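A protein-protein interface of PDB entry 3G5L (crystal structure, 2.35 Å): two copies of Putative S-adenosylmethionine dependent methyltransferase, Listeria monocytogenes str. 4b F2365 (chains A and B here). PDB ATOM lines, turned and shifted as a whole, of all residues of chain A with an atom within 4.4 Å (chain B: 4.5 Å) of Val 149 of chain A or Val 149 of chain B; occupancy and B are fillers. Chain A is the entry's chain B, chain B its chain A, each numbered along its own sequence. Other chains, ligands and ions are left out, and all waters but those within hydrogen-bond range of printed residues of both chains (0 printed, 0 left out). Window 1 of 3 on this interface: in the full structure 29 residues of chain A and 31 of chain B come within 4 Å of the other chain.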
ATOM      1  N   HIS A 147      10.023 -21.875  -2.696  1.00  0.00           N
ATOM      2  CA  HIS A 147       9.943 -22.705  -3.888  1.00  0.00           C
ATOM      3  C   HIS A 147       9.593 -21.826  -5.084  1.00  0.00           C
ATOM      4  O   HIS A 147       8.777 -20.918  -4.953  1.00  0.00           O
ATOM      5  CB  HIS A 147       8.876 -23.788  -3.689  1.00  0.00           C
ATOM      6  CG  HIS A 147       9.013 -24.960  -4.609  1.00  0.00           C
ATOM      7  ND1 HIS A 147       8.709 -24.891  -5.952  1.00  0.00           N
ATOM      8  CD2 HIS A 147       9.405 -26.236  -4.375  1.00  0.00           C
ATOM      9  CE1 HIS A 147       8.932 -26.069  -6.511  1.00  0.00           C
ATOM     10  NE2 HIS A 147       9.350 -26.902  -5.576  1.00  0.00           N
ATOM     11  N   PRO A 148      10.250 -22.060  -6.235  1.00  0.00           N
ATOM     12  CA  PRO A 148       9.924 -21.449  -7.534  1.00  0.00           C
ATOM     13  C   PRO A 148       8.426 -21.361  -7.880  1.00  0.00           C
ATOM     14  O   PRO A 148       8.005 -20.378  -8.474  1.00  0.00           O
ATOM     15  CB  PRO A 148      10.661 -22.354  -8.517  1.00  0.00           C
ATOM     16  CG  PRO A 148      11.894 -22.753  -7.752  1.00  0.00           C
ATOM     17  CD  PRO A 148      11.451 -22.916  -6.326  1.00  0.00           C
ATOM     18  N   VAL A 149       7.649 -22.372  -7.490  1.00  0.00           N
ATOM     19  CA  VAL A 149       6.190 -22.404  -7.659  1.00  0.00           C
ATOM     20  C   VAL A 149       5.456 -21.376  -6.776  1.00  0.00           C
ATOM     21  O   VAL A 149       4.420 -20.830  -7.174  1.00  0.00           O
ATOM     22  CB  VAL A 149       5.656 -23.842  -7.422  1.00  0.00           C
ATOM     23  CG1 VAL A 149       4.115 -23.901  -7.396  1.00  0.00           C
ATOM     24  CG2 VAL A 149       6.209 -24.773  -8.491  1.00  0.00           C
ATOM     25  N   PHE A 150       5.997 -21.114  -5.588  1.00  0.00           N
ATOM     26  CA  PHE A 150       5.496 -20.038  -4.723  1.00  0.00           C
ATOM     27  C   PHE A 150       5.815 -18.644  -5.293  1.00  0.00           C
ATOM     28  O   PHE A 150       5.026 -17.706  -5.129  1.00  0.00           O
ATOM     29  CB  PHE A 150       6.059 -20.183  -3.296  1.00  0.00           C
ATOM     30  CG  PHE A 150       5.555 -19.150  -2.329  1.00  0.00           C
ATOM     31  CD1 PHE A 150       4.388 -19.364  -1.618  1.00  0.00           C
ATOM     32  CD2 PHE A 150       6.251 -17.966  -2.119  1.00  0.00           C
ATOM     33  CE1 PHE A 150       3.917 -18.410  -0.731  1.00  0.00           C
ATOM     34  CE2 PHE A 150       5.785 -17.008  -1.241  1.00  0.00           C
ATOM     35  CZ  PHE A 150       4.616 -17.228  -0.548  1.00  0.00           C
ATOM     36  N   THR A 151       6.962 -18.516  -5.961  1.00  0.00           N
ATOM     37  CA  THR A 151       7.470 -17.205  -6.390  1.00  0.00           C
ATOM     38  C   THR A 151       7.212 -16.843  -7.858  1.00  0.00           C
ATOM     39  O   THR A 151       7.428 -15.695  -8.247  1.00  0.00           O
ATOM     40  CB  THR A 151       8.999 -17.058  -6.125  1.00  0.00           C
ATOM     41  OG1 THR A 151       9.716 -18.078  -6.834  1.00  0.00           O
ATOM     42  CG2 THR A 151       9.314 -17.146  -4.645  1.00  0.00           C
ATOM     43  N   ALA A 152       6.762 -17.808  -8.661  1.00  0.00           N
ATOM     44  CA  ALA A 152       6.641 -17.633 -10.117  1.00  0.00           C
ATOM     45  C   ALA A 152       5.693 -16.511 -10.543  1.00  0.00           C
ATOM     46  O   ALA A 152       6.104 -15.560 -11.224  1.00  0.00           O
ATOM     47  CB  ALA A 152       6.238 -18.956 -10.789  1.00  0.00           C
ATOM     48  N   TRP A 169      -3.562 -23.038  -6.591  1.00  0.00           N
ATOM     49  CA  TRP A 169      -2.440 -22.126  -6.575  1.00  0.00           C
ATOM     50  C   TRP A 169      -2.066 -21.747  -8.008  1.00  0.00           C
ATOM     51  O   TRP A 169      -1.858 -22.620  -8.846  1.00  0.00           O
ATOM     52  CB  TRP A 169      -1.248 -22.764  -5.857  1.00  0.00           C
ATOM     53  CG  TRP A 169      -0.111 -21.821  -5.621  1.00  0.00           C
ATOM     54  CD1 TRP A 169       0.977 -21.625  -6.427  1.00  0.00           C
ATOM     55  CD2 TRP A 169       0.051 -20.937  -4.505  1.00  0.00           C
ATOM     56  NE1 TRP A 169       1.816 -20.685  -5.873  1.00  0.00           N
ATOM     57  CE2 TRP A 169       1.269 -20.244  -4.695  1.00  0.00           C
ATOM     58  CE3 TRP A 169      -0.712 -20.669  -3.358  1.00  0.00           C
ATOM     59  CZ2 TRP A 169       1.737 -19.292  -3.788  1.00  0.00           C
ATOM     60  CZ3 TRP A 169      -0.242 -19.732  -2.449  1.00  0.00           C
ATOM     61  CH2 TRP A 169       0.977 -19.055  -2.671  1.00  0.00           C
ATOM     62  N   VAL A 171       0.188 -20.509 -11.107  1.00  0.00           N
ATOM     63  CA  VAL A 171       1.548 -20.430 -11.642  1.00  0.00           C
ATOM     64  C   VAL A 171       1.517 -19.638 -12.938  1.00  0.00           C
ATOM     65  O   VAL A 171       0.661 -19.866 -13.795  1.00  0.00           O
ATOM     66  CB  VAL A 171       2.164 -21.838 -11.871  1.00  0.00           C
ATOM     67  CG1 VAL A 171       3.502 -21.765 -12.628  1.00  0.00           C
ATOM     68  CG2 VAL A 171       2.379 -22.523 -10.546  1.00  0.00           C
ATOM     69  N   PRO A 235       3.787 -26.670  -3.244  1.00  0.00           N
ATOM     70  CA  PRO A 235       5.034 -26.623  -2.474  1.00  0.00           C
ATOM     71  C   PRO A 235       5.424 -25.195  -2.087  1.00  0.00           C
ATOM     72  O   PRO A 235       5.293 -24.260  -2.888  1.00  0.00           O
ATOM     73  CB  PRO A 235       6.064 -27.234  -3.433  1.00  0.00           C
ATOM     74  CG  PRO A 235       5.555 -26.896  -4.808  1.00  0.00           C
ATOM     75  CD  PRO A 235       4.039 -26.766  -4.699  1.00  0.00           C
ATOM     76  N   HIS B 147       6.141 -32.583 -16.543  1.00  0.00           N
ATOM     77  CA  HIS B 147       6.535 -31.940 -15.299  1.00  0.00           C
ATOM     78  C   HIS B 147       5.507 -32.190 -14.197  1.00  0.00           C
ATOM     79  O   HIS B 147       4.308 -32.233 -14.478  1.00  0.00           O
ATOM     80  CB  HIS B 147       6.708 -30.437 -15.534  1.00  0.00           C
ATOM     81  CG  HIS B 147       7.591 -29.756 -14.531  1.00  0.00           C
ATOM     82  ND1 HIS B 147       7.148 -29.372 -13.288  1.00  0.00           N
ATOM     83  CD2 HIS B 147       8.888 -29.374 -14.600  1.00  0.00           C
ATOM     84  CE1 HIS B 147       8.129 -28.784 -12.629  1.00  0.00           C
ATOM     85  NE2 HIS B 147       9.199 -28.776 -13.403  1.00  0.00           N
ATOM     86  N   PRO B 148       5.978 -32.423 -12.955  1.00  0.00           N
ATOM     87  CA  PRO B 148       5.102 -32.432 -11.767  1.00  0.00           C
ATOM     88  C   PRO B 148       4.087 -31.286 -11.690  1.00  0.00           C
ATOM     89  O   PRO B 148       2.950 -31.530 -11.303  1.00  0.00           O
ATOM     90  CB  PRO B 148       6.097 -32.362 -10.610  1.00  0.00           C
ATOM     91  CG  PRO B 148       7.288 -33.173 -11.143  1.00  0.00           C
ATOM     92  CD  PRO B 148       7.375 -32.777 -12.609  1.00  0.00           C
ATOM     93  N   VAL B 149       4.493 -30.073 -12.075  1.00  0.00           N
ATOM     94  CA  VAL B 149       3.603 -28.903 -12.173  1.00  0.00           C
ATOM     95  C   VAL B 149       2.536 -29.070 -13.271  1.00  0.00           C
ATOM     96  O   VAL B 149       1.417 -28.583 -13.132  1.00  0.00           O
ATOM     97  CB  VAL B 149       4.421 -27.572 -12.357  1.00  0.00           C
ATOM     98  CG1 VAL B 149       3.564 -26.406 -12.902  1.00  0.00           C
ATOM     99  CG2 VAL B 149       5.085 -27.175 -11.053  1.00  0.00           C
ATOM    100  N   PHE B 150       2.886 -29.763 -14.353  1.00  0.00           N
ATOM    101  CA  PHE B 150       1.911 -30.093 -15.393  1.00  0.00           C
ATOM    102  C   PHE B 150       0.848 -31.100 -14.916  1.00  0.00           C
ATOM    103  O   PHE B 150      -0.321 -30.989 -15.278  1.00  0.00           O
ATOM    104  CB  PHE B 150       2.625 -30.605 -16.655  1.00  0.00           C
ATOM    105  CG  PHE B 150       1.724 -30.768 -17.841  1.00  0.00           C
ATOM    106  CD1 PHE B 150       1.405 -29.675 -18.642  1.00  0.00           C
ATOM    107  CD2 PHE B 150       1.186 -32.013 -18.158  1.00  0.00           C
ATOM    108  CE1 PHE B 150       0.554 -29.820 -19.751  1.00  0.00           C
ATOM    109  CE2 PHE B 150       0.329 -32.169 -19.258  1.00  0.00           C
ATOM    110  CZ  PHE B 150       0.015 -31.071 -20.057  1.00  0.00           C
ATOM    111  N   THR B 151       1.255 -32.066 -14.095  1.00  0.00           N
ATOM    112  CA  THR B 151       0.382 -33.181 -13.728  1.00  0.00           C
ATOM    113  C   THR B 151      -0.329 -32.986 -12.399  1.00  0.00           C
ATOM    114  O   THR B 151      -1.301 -33.685 -12.118  1.00  0.00           O
ATOM    115  CB  THR B 151       1.142 -34.532 -13.670  1.00  0.00           C
ATOM    116  OG1 THR B 151       2.258 -34.420 -12.779  1.00  0.00           O
ATOM    117  CG2 THR B 151       1.625 -34.949 -15.035  1.00  0.00           C
ATOM    118  N   ALA B 152       0.154 -32.038 -11.595  1.00  0.00           N
ATOM    119  CA  ALA B 152      -0.311 -31.859 -10.214  1.00  0.00           C
ATOM    120  C   ALA B 152      -1.818 -31.723 -10.056  1.00  0.00           C
ATOM    121  O   ALA B 152      -2.435 -32.532  -9.359  1.00  0.00           O
ATOM    122  CB  ALA B 152       0.417 -30.693  -9.535  1.00  0.00           C
ATOM    123  N   TRP B 169      -1.619 -20.936 -14.901  1.00  0.00           N
ATOM    124  CA  TRP B 169      -1.612 -22.388 -14.793  1.00  0.00           C
ATOM    125  C   TRP B 169      -1.936 -22.803 -13.357  1.00  0.00           C
ATOM    126  O   TRP B 169      -1.208 -22.442 -12.439  1.00  0.00           O
ATOM    127  CB  TRP B 169      -0.249 -22.952 -15.204  1.00  0.00           C
ATOM    128  CG  TRP B 169      -0.245 -24.451 -15.272  1.00  0.00           C
ATOM    129  CD1 TRP B 169       0.121 -25.321 -14.282  1.00  0.00           C
ATOM    130  CD2 TRP B 169      -0.654 -25.256 -16.379  1.00  0.00           C
ATOM    131  NE1 TRP B 169      -0.024 -26.613 -14.713  1.00  0.00           N
ATOM    132  CE2 TRP B 169      -0.502 -26.603 -15.996  1.00  0.00           C
ATOM    133  CE3 TRP B 169      -1.125 -24.969 -17.664  1.00  0.00           C
ATOM    134  CZ2 TRP B 169      -0.811 -27.658 -16.845  1.00  0.00           C
ATOM    135  CZ3 TRP B 169      -1.424 -26.021 -18.510  1.00  0.00           C
ATOM    136  CH2 TRP B 169      -1.265 -27.344 -18.098  1.00  0.00           C
ATOM    137  N   VAL B 171      -2.206 -25.063 -10.037  1.00  0.00           N
ATOM    138  CA  VAL B 171      -1.507 -26.131  -9.328  1.00  0.00           C
ATOM    139  C   VAL B 171      -2.331 -26.494  -8.091  1.00  0.00           C
ATOM    140  O   VAL B 171      -2.755 -25.613  -7.347  1.00  0.00           O
ATOM    141  CB  VAL B 171      -0.044 -25.716  -8.960  1.00  0.00           C
ATOM    142  CG1 VAL B 171       0.562 -26.629  -7.916  1.00  0.00           C
ATOM    143  CG2 VAL B 171       0.830 -25.720 -10.199  1.00  0.00           C
ATOM    144  N   TYR B 174      -0.352 -31.155  -4.995  1.00  0.00           N
ATOM    145  CA  TYR B 174       1.013 -31.355  -5.462  1.00  0.00           C
ATOM    146  C   TYR B 174       1.702 -32.536  -4.794  1.00  0.00           C
ATOM    147  O   TYR B 174       2.528 -33.211  -5.412  1.00  0.00           O
ATOM    148  CB  TYR B 174       1.849 -30.076  -5.308  1.00  0.00           C
ATOM    149  CG  TYR B 174       3.243 -30.213  -5.879  1.00  0.00           C
ATOM    150  CD1 TYR B 174       3.476 -30.082  -7.253  1.00  0.00           C
ATOM    151  CD2 TYR B 174       4.326 -30.504  -5.051  1.00  0.00           C
ATOM    152  CE1 TYR B 174       4.767 -30.233  -7.780  1.00  0.00           C
ATOM    153  CE2 TYR B 174       5.610 -30.656  -5.570  1.00  0.00           C
ATOM    154  CZ  TYR B 174       5.824 -30.524  -6.925  1.00  0.00           C
ATOM    155  OH  TYR B 174       7.105 -30.673  -7.407  1.00  0.00           O
ATOM    156  N   PRO B 235       6.277 -24.795 -16.663  1.00  0.00           N
ATOM    157  CA  PRO B 235       7.032 -25.874 -17.306  1.00  0.00           C
ATOM    158  C   PRO B 235       6.146 -27.081 -17.679  1.00  0.00           C
ATOM    159  O   PRO B 235       5.335 -27.541 -16.868  1.00  0.00           O
ATOM    160  CB  PRO B 235       8.067 -26.239 -16.253  1.00  0.00           C
ATOM    161  CG  PRO B 235       7.423 -25.908 -14.948  1.00  0.00           C
ATOM    162  CD  PRO B 235       6.428 -24.808 -15.194  1.00  0.00           C
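Among the printed residues, merely in contact across the chains: Val 171 of chain A with Val 171 of chain B, Trp 169 of chain A with Trp 169 of chain B, Val 149 of chain A with Val 149 of chain B and Pro 235 of chain A with Tyr 174 of chain B.
The backbone carbonyl oxygen of Val 149 of chain A lies within hydrogen-bond range of the indole nitrogen of Trp 169 of chain A, 2.9 Å away.
O of Val 149 of chain B sits at hydrogen-bond distance from NE1 of Trp 169 of chain B.
The backbone NH (N) of Val 149 of chain A lies within hydrogen-bond range of a ring nitrogen (ND1) of His 147 of chain A (3.1 Å).
ND1 of His 147 of chain B lies within hydrogen-bond range of N of Val 149 of chain B, 3.0 Å away.
The backbone NH (N) of Val 171 of chain B lies within hydrogen-bond range of the backbone carbonyl oxygen (O) of Trp 169 of chain A, 2.7 Å away.
O of Trp 169 of chain B sits at hydrogen-bond distance from N of Val 171 of chain A (2.7 Å).
Val 149 of chain B touches its own counterpart, Val 149 of chain A.
Trp 169 of chain A touches its own counterpart, Trp 169 of chain B.
Trp 169 of chain A touches Val 171 of chain B, and with the chains exchanged Val 171 of chain A touches Trp 169 of chain B.
Val 171 of chain A touches its own counterpart, Val 171 of chain B.
Positions printed for both chains: 147, 148, 149, 150, 151, 152, 169, 171 and 235.
Of the 6 pairs that touch across the chains among the printed residues, 5 have their exchanged pair printed and touching as well.
Of the printed residues of chain B, Val 149 of chain A touches Val 149.
Ala 152 of chain A touches none of the printed residues of chain B.
Of the printed residues of chain B, Trp 169 of chain A touches Trp 169 (3.7 Å) and Val 171 (2.7 Å).
Of the printed residues of chain B, Val 171 of chain A touches Trp 169 (2.7 Å) and Val 171 (3.6 Å).
Of the printed residues of chain B, Pro 235 of chain A touches Tyr 174.
Of chain A, only Val 149 (3.7 Å) comes within 4 Å of Val 149 of chain B.
Printed residues of chain A within 4 Å of Tyr 174 of chain B: Pro 235 (3.7 Å).
The nearest printed residue of chain B that does not touch Val 149 of chain A is Val 171 of chain B (4.5 Å).
The nearest printed residue of chain B that does not touch Pro 235 of chain A is Val 171 of chain B (4.7 Å).
Of the 10 printed residues of chain B, 4 touch a printed residue of chain A.
Of the 9 printed residues of chain A, 4 touch a printed residue of chain B.
Among the printed residues, no Asp or Glu carboxylate lies within 4 Å of a Lys or Arg side-chain nitrogen of the other chain.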
